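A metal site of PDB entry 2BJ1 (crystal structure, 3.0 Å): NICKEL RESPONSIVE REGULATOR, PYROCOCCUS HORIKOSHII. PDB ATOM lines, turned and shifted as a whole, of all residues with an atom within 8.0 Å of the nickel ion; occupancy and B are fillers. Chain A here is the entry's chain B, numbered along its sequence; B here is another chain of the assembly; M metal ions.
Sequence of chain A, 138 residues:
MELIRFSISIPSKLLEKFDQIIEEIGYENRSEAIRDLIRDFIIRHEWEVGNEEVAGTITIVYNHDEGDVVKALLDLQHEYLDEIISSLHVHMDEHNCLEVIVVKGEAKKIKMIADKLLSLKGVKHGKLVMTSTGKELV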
ATOM      1  N   TYR A  62     -10.499   5.536 -13.048  1.00  0.00           N
ATOM      2  CA  TYR A  62      -9.967   4.183 -13.157  1.00  0.00           C
ATOM      3  C   TYR A  62      -9.013   3.843 -12.010  1.00  0.00           C
ATOM      4  O   TYR A  62      -8.288   4.698 -11.508  1.00  0.00           O
ATOM      5  CB  TYR A  62      -9.225   4.042 -14.483  1.00  0.00           C
ATOM      6  CG  TYR A  62      -7.994   4.912 -14.590  1.00  0.00           C
ATOM      7  CD1 TYR A  62      -6.755   4.451 -14.162  1.00  0.00           C
ATOM      8  CD2 TYR A  62      -8.077   6.209 -15.108  1.00  0.00           C
ATOM      9  CE1 TYR A  62      -5.622   5.266 -14.222  1.00  0.00           C
ATOM     10  CE2 TYR A  62      -6.953   7.030 -15.177  1.00  0.00           C
ATOM     11  CZ  TYR A  62      -5.726   6.553 -14.738  1.00  0.00           C
ATOM     12  OH  TYR A  62      -4.601   7.353 -14.801  1.00  0.00           O
ATOM     13  N   HIS A  64      -5.880   2.769 -11.165  1.00  0.00           N
ATOM     14  CA  HIS A  64      -4.604   2.574 -11.845  1.00  0.00           C
ATOM     15  C   HIS A  64      -3.914   1.243 -11.578  1.00  0.00           C
ATOM     16  O   HIS A  64      -3.034   0.844 -12.345  1.00  0.00           O
ATOM     17  CB  HIS A  64      -3.644   3.721 -11.508  1.00  0.00           C
ATOM     18  CG  HIS A  64      -3.274   3.811 -10.065  1.00  0.00           C
ATOM     19  ND1 HIS A  64      -4.194   4.107  -9.082  1.00  0.00           N
ATOM     20  CD2 HIS A  64      -2.090   3.635  -9.435  1.00  0.00           C
ATOM     21  CE1 HIS A  64      -3.588   4.125  -7.907  1.00  0.00           C
ATOM     22  NE2 HIS A  64      -2.307   3.840  -8.093  1.00  0.00           N
ATOM     23  N   VAL A  70      -2.904   2.012 -16.644  1.00  0.00           N
ATOM     24  CA  VAL A  70      -2.055   3.203 -16.646  1.00  0.00           C
ATOM     25  C   VAL A  70      -1.135   3.179 -17.845  1.00  0.00           C
ATOM     26  O   VAL A  70      -0.844   4.217 -18.457  1.00  0.00           O
ATOM     27  CB  VAL A  70      -1.173   3.272 -15.393  1.00  0.00           C
ATOM     28  CG1 VAL A  70      -0.404   4.591 -15.372  1.00  0.00           C
ATOM     29  CG2 VAL A  70      -2.031   3.105 -14.154  1.00  0.00           C
ATOM     30  N   HIS A  89      -4.999  15.204 -14.457  1.00  0.00           N
ATOM     31  CA  HIS A  89      -5.117  13.995 -13.648  1.00  0.00           C
ATOM     32  C   HIS A  89      -5.159  14.314 -12.165  1.00  0.00           C
ATOM     33  O   HIS A  89      -4.232  14.900 -11.621  1.00  0.00           O
ATOM     34  CB  HIS A  89      -3.942  13.055 -13.963  1.00  0.00           C
ATOM     35  CG  HIS A  89      -3.844  11.857 -13.078  1.00  0.00           C
ATOM     36  ND1 HIS A  89      -3.591  10.592 -13.573  1.00  0.00           N
ATOM     37  CD2 HIS A  89      -3.890  11.722 -11.728  1.00  0.00           C
ATOM     38  CE1 HIS A  89      -3.485   9.741 -12.563  1.00  0.00           C
ATOM     39  NE2 HIS A  89      -3.661  10.402 -11.428  1.00  0.00           N
ATOM     40  N   VAL A  90      -6.236  13.918 -11.507  1.00  0.00           N
ATOM     41  CA  VAL A  90      -6.397  14.149 -10.085  1.00  0.00           C
ATOM     42  C   VAL A  90      -6.471  12.828  -9.342  1.00  0.00           C
ATOM     43  O   VAL A  90      -7.412  12.065  -9.534  1.00  0.00           O
ATOM     44  CB  VAL A  90      -7.677  14.953  -9.804  1.00  0.00           C
ATOM     45  CG1 VAL A  90      -8.001  14.924  -8.338  1.00  0.00           C
ATOM     46  CG2 VAL A  90      -7.501  16.392 -10.284  1.00  0.00           C
ATOM     47  N   HIS A  91      -5.480  12.567  -8.485  1.00  0.00           N
ATOM     48  CA  HIS A  91      -5.414  11.332  -7.690  1.00  0.00           C
ATOM     49  C   HIS A  91      -6.515  11.348  -6.646  1.00  0.00           C
ATOM     50  O   HIS A  91      -6.357  11.952  -5.590  1.00  0.00           O
ATOM     51  CB  HIS A  91      -4.072  11.252  -6.975  1.00  0.00           C
ATOM     52  CG  HIS A  91      -2.885  11.431  -7.861  1.00  0.00           C
ATOM     53  ND1 HIS A  91      -2.589  10.574  -8.893  1.00  0.00           N
ATOM     54  CD2 HIS A  91      -1.912  12.371  -7.864  1.00  0.00           C
ATOM     55  CE1 HIS A  91      -1.474  10.977  -9.492  1.00  0.00           C
ATOM     56  NE2 HIS A  91      -1.041  12.063  -8.887  1.00  0.00           N
ATOM     57  N   MET A  92      -7.625  10.671  -6.933  1.00  0.00           N
ATOM     58  CA  MET A  92      -8.774  10.642  -6.026  1.00  0.00           C
ATOM     59  C   MET A  92      -8.542   9.952  -4.671  1.00  0.00           C
ATOM     60  O   MET A  92      -9.131  10.345  -3.654  1.00  0.00           O
ATOM     61  CB  MET A  92      -9.961  10.001  -6.739  1.00  0.00           C
ATOM     62  CG  MET A  92     -10.525  10.861  -7.847  1.00  0.00           C
ATOM     63  SD  MET A  92     -11.472  12.273  -7.211  1.00  0.00           S
ATOM     64  CE  MET A  92     -10.198  13.413  -6.648  1.00  0.00           C
ATOM     65  N   ASP A  93      -7.704   8.917  -4.674  1.00  0.00           N
ATOM     66  CA  ASP A  93      -7.382   8.179  -3.463  1.00  0.00           C
ATOM     67  C   ASP A  93      -6.244   7.200  -3.746  1.00  0.00           C
ATOM     68  O   ASP A  93      -5.793   7.083  -4.878  1.00  0.00           O
ATOM     69  CB  ASP A  93      -8.603   7.418  -2.931  1.00  0.00           C
ATOM     70  CG  ASP A  93      -8.940   6.197  -3.766  1.00  0.00           C
ATOM     71  OD1 ASP A  93      -8.066   5.319  -3.915  1.00  0.00           O
ATOM     72  OD2 ASP A  93     -10.084   6.117  -4.278  1.00  0.00           O
ATOM     73  N   GLU A  94      -5.797   6.494  -2.709  1.00  0.00           N
ATOM     74  CA  GLU A  94      -4.698   5.565  -2.865  1.00  0.00           C
ATOM     75  C   GLU A  94      -4.756   4.686  -4.104  1.00  0.00           C
ATOM     76  O   GLU A  94      -3.717   4.362  -4.686  1.00  0.00           O
ATOM     77  CB  GLU A  94      -4.619   4.650  -1.633  1.00  0.00           C
ATOM     78  CG  GLU A  94      -3.431   3.709  -1.648  1.00  0.00           C
ATOM     79  CD  GLU A  94      -3.635   2.472  -0.794  1.00  0.00           C
ATOM     80  OE1 GLU A  94      -2.673   1.694  -0.619  1.00  0.00           O
ATOM     81  OE2 GLU A  94      -4.767   2.280  -0.290  1.00  0.00           O
ATOM     82  N   HIS A  95      -5.965   4.315  -4.524  1.00  0.00           N
ATOM     83  CA  HIS A  95      -6.157   3.431  -5.662  1.00  0.00           C
ATOM     84  C   HIS A  95      -6.865   3.992  -6.890  1.00  0.00           C
ATOM     85  O   HIS A  95      -6.641   3.530  -8.013  1.00  0.00           O
ATOM     86  CB  HIS A  95      -6.932   2.180  -5.214  1.00  0.00           C
ATOM     87  CG  HIS A  95      -6.164   1.290  -4.284  1.00  0.00           C
ATOM     88  ND1 HIS A  95      -5.088   0.534  -4.699  1.00  0.00           N
ATOM     89  CD2 HIS A  95      -6.319   1.028  -2.968  1.00  0.00           C
ATOM     90  CE1 HIS A  95      -4.617  -0.149  -3.669  1.00  0.00           C
ATOM     91  NE2 HIS A  95      -5.350   0.134  -2.612  1.00  0.00           N
ATOM     92  N   ASN A  96      -7.719   4.990  -6.691  1.00  0.00           N
ATOM     93  CA  ASN A  96      -8.466   5.568  -7.795  1.00  0.00           C
ATOM     94  C   ASN A  96      -7.993   6.899  -8.366  1.00  0.00           C
ATOM     95  O   ASN A  96      -7.524   7.793  -7.647  1.00  0.00           O
ATOM     96  CB  ASN A  96      -9.934   5.649  -7.412  1.00  0.00           C
ATOM     97  CG  ASN A  96     -10.644   4.343  -7.622  1.00  0.00           C
ATOM     98  OD1 ASN A  96     -10.946   3.970  -8.755  1.00  0.00           O
ATOM     99  ND2 ASN A  96     -10.910   3.631  -6.535  1.00  0.00           N
ATOM    100  N   CYS A  97      -8.146   7.020  -9.694  1.00  0.00           N
ATOM    101  CA  CYS A  97      -7.752   8.202 -10.439  1.00  0.00           C
ATOM    102  C   CYS A  97      -8.882   8.818 -11.266  1.00  0.00           C
ATOM    103  O   CYS A  97      -9.706   8.103 -11.821  1.00  0.00           O
ATOM    104  CB  CYS A  97      -6.596   7.872 -11.381  1.00  0.00           C
ATOM    105  SG  CYS A  97      -5.030   7.565 -10.566  1.00  0.00           S
ATOM    106  N   LEU A  98      -8.896  10.141 -11.347  1.00  0.00           N
ATOM    107  CA  LEU A  98      -9.862  10.865 -12.166  1.00  0.00           C
ATOM    108  C   LEU A  98      -8.945  11.579 -13.151  1.00  0.00           C
ATOM    109  O   LEU A  98      -7.986  12.243 -12.753  1.00  0.00           O
ATOM    110  CB  LEU A  98     -10.654  11.877 -11.321  1.00  0.00           C
ATOM    111  CG  LEU A  98     -11.872  12.543 -11.982  1.00  0.00           C
ATOM    112  CD1 LEU A  98     -12.497  13.524 -11.010  1.00  0.00           C
ATOM    113  CD2 LEU A  98     -11.457  13.266 -13.240  1.00  0.00           C
ATOM    114  N   GLU A  99      -9.228  11.455 -14.433  1.00  0.00           N
ATOM    115  CA  GLU A  99      -8.368  12.088 -15.423  1.00  0.00           C
ATOM    116  C   GLU A  99      -9.211  12.599 -16.561  1.00  0.00           C
ATOM    117  O   GLU A  99      -9.948  11.836 -17.188  1.00  0.00           O
ATOM    118  CB  GLU A  99      -7.339  11.067 -15.928  1.00  0.00           C
ATOM    119  CG  GLU A  99      -6.272  11.631 -16.850  1.00  0.00           C
ATOM    120  CD  GLU A  99      -5.264  10.579 -17.311  1.00  0.00           C
ATOM    121  OE1 GLU A  99      -4.656   9.901 -16.455  1.00  0.00           O
ATOM    122  OE2 GLU A  99      -5.067  10.444 -18.543  1.00  0.00           O
ATOM    123  N   LEU B  73       5.710   6.763 -10.390  1.00  0.00           N
ATOM    124  CA  LEU B  73       5.217   8.113 -10.171  1.00  0.00           C
ATOM    125  C   LEU B  73       3.855   8.103  -9.505  1.00  0.00           C
ATOM    126  O   LEU B  73       3.659   8.743  -8.470  1.00  0.00           O
ATOM    127  CB  LEU B  73       5.127   8.857 -11.492  1.00  0.00           C
ATOM    128  CG  LEU B  73       6.392   9.652 -11.786  1.00  0.00           C
ATOM    129  CD1 LEU B  73       6.623   9.825 -13.275  1.00  0.00           C
ATOM    130  CD2 LEU B  73       6.279  10.984 -11.081  1.00  0.00           C
ATOM    131  N   LEU B  74       2.908   7.387 -10.108  1.00  0.00           N
ATOM    132  CA  LEU B  74       1.565   7.297  -9.560  1.00  0.00           C
ATOM    133  C   LEU B  74       1.563   6.721  -8.151  1.00  0.00           C
ATOM    134  O   LEU B  74       0.965   7.295  -7.236  1.00  0.00           O
ATOM    135  CB  LEU B  74       0.646   6.457 -10.465  1.00  0.00           C
ATOM    136  CG  LEU B  74       0.039   7.153 -11.704  1.00  0.00           C
ATOM    137  CD1 LEU B  74      -0.930   6.194 -12.382  1.00  0.00           C
ATOM    138  CD2 LEU B  74      -0.702   8.425 -11.312  1.00  0.00           C
ATOM    139  N   ASP B  75       2.250   5.597  -7.961  1.00  0.00           N
ATOM    140  CA  ASP B  75       2.318   4.975  -6.650  1.00  0.00           C
ATOM    141  C   ASP B  75       2.874   5.979  -5.656  1.00  0.00           C
ATOM    142  O   ASP B  75       2.320   6.158  -4.576  1.00  0.00           O
ATOM    143  CB  ASP B  75       3.206   3.731  -6.695  1.00  0.00           C
ATOM    144  CG  ASP B  75       2.605   2.620  -7.541  1.00  0.00           C
ATOM    145  OD1 ASP B  75       1.527   2.098  -7.191  1.00  0.00           O
ATOM    146  OD2 ASP B  75       3.239   2.269  -8.560  1.00  0.00           O
ATOM    147  N   GLN B  77       3.187   9.440  -5.936  1.00  0.00           N
ATOM    148  CA  GLN B  77       2.261  10.558  -5.764  1.00  0.00           C
ATOM    149  C   GLN B  77       1.029  10.182  -4.941  1.00  0.00           C
ATOM    150  O   GLN B  77       0.700  10.869  -3.974  1.00  0.00           O
ATOM    151  CB  GLN B  77       1.840  11.095  -7.136  1.00  0.00           C
ATOM    152  CG  GLN B  77       2.998  11.658  -7.945  1.00  0.00           C
ATOM    153  CD  GLN B  77       2.554  12.473  -9.131  1.00  0.00           C
ATOM    154  OE1 GLN B  77       1.798  13.427  -8.987  1.00  0.00           O
ATOM    155  NE2 GLN B  77       3.018  12.098 -10.319  1.00  0.00           N
ATOM    156  N   HIS B  78       0.378   9.087  -5.302  1.00  0.00           N
ATOM    157  CA  HIS B  78      -0.800   8.646  -4.575  1.00  0.00           C
ATOM    158  C   HIS B  78      -0.498   8.408  -3.087  1.00  0.00           C
ATOM    159  O   HIS B  78      -1.412   8.265  -2.271  1.00  0.00           O
ATOM    160  CB  HIS B  78      -1.362   7.357  -5.217  1.00  0.00           C
ATOM    161  CG  HIS B  78      -2.307   7.603  -6.355  1.00  0.00           C
ATOM    162  ND1 HIS B  78      -3.620   7.972  -6.161  1.00  0.00           N
ATOM    163  CD2 HIS B  78      -2.119   7.561  -7.689  1.00  0.00           C
ATOM    164  CE1 HIS B  78      -4.206   8.150  -7.330  1.00  0.00           C
ATOM    165  NE2 HIS B  78      -3.318   7.906  -8.286  1.00  0.00           N
ATOM    166  N   LEU B  81      -1.272  12.094  -1.114  1.00  0.00           N
ATOM    167  CA  LEU B  81      -2.430  12.756  -1.689  1.00  0.00           C
ATOM    168  C   LEU B  81      -2.543  14.174  -1.173  1.00  0.00           C
ATOM    169  O   LEU B  81      -2.485  15.125  -1.937  1.00  0.00           O
ATOM    170  CB  LEU B  81      -3.704  11.990  -1.351  1.00  0.00           C
ATOM    171  CG  LEU B  81      -3.817  10.621  -2.012  1.00  0.00           C
ATOM    172  CD1 LEU B  81      -5.121   9.964  -1.627  1.00  0.00           C
ATOM    173  CD2 LEU B  81      -3.731  10.772  -3.519  1.00  0.00           C
ATOM    174  N   SER B  87      -2.356  17.672 -11.583  1.00  0.00           N
ATOM    175  CA  SER B  87      -1.154  17.673 -12.393  1.00  0.00           C
ATOM    176  C   SER B  87      -1.449  17.595 -13.870  1.00  0.00           C
ATOM    177  O   SER B  87      -2.100  16.675 -14.325  1.00  0.00           O
ATOM    178  CB  SER B  87      -0.255  16.505 -12.017  1.00  0.00           C
ATOM    179  OG  SER B  87      -0.724  15.315 -12.608  1.00  0.00           O
HETATM  180 NI    NI M   1      -3.625   9.208  -9.765  1.00  0.00          NI
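Merely in contact with the nickel ion: Leu 74 of chain B.
Of the 21 residues printed, 5 come within 4 Å of the nickel ion.
The nearest printed residue that does not touch the nickel ion is Val 90 (4.6 Å).
The nickel ion is bound by a ring nitrogen (ND1) of His 91, at 1.9 Å.
The nickel ion is bound by NE2 of His 78 of chain B (2.0 Å).
The nickel ion is bound by NE2 of His 89, 2.0 Å away.
SG of Cys 97 is bound to the nickel ion.
The nickel ion has four donor atoms within binding distance.
A ring nitrogen (NE2) of His 91 lies within hydrogen-bond range of the side-chain amide oxygen (OE1) of Gln 77 of chain B.
A ring nitrogen (ND1) of His 78 of chain B lies within hydrogen-bond range of the backbone carbonyl oxygen of Asp 93 (2.7 Å).
ND1 of His 89 is in hydrogen-bond range of OE1 of Glu 99.
The backbone NH (N) of His 89 sits at hydrogen-bond distance from the backbone carbonyl oxygen (O) of Ser 87 of chain B (3.3 Å).
O of Tyr 62 sits at hydrogen-bond distance from N of Cys 97 (2.9 Å).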
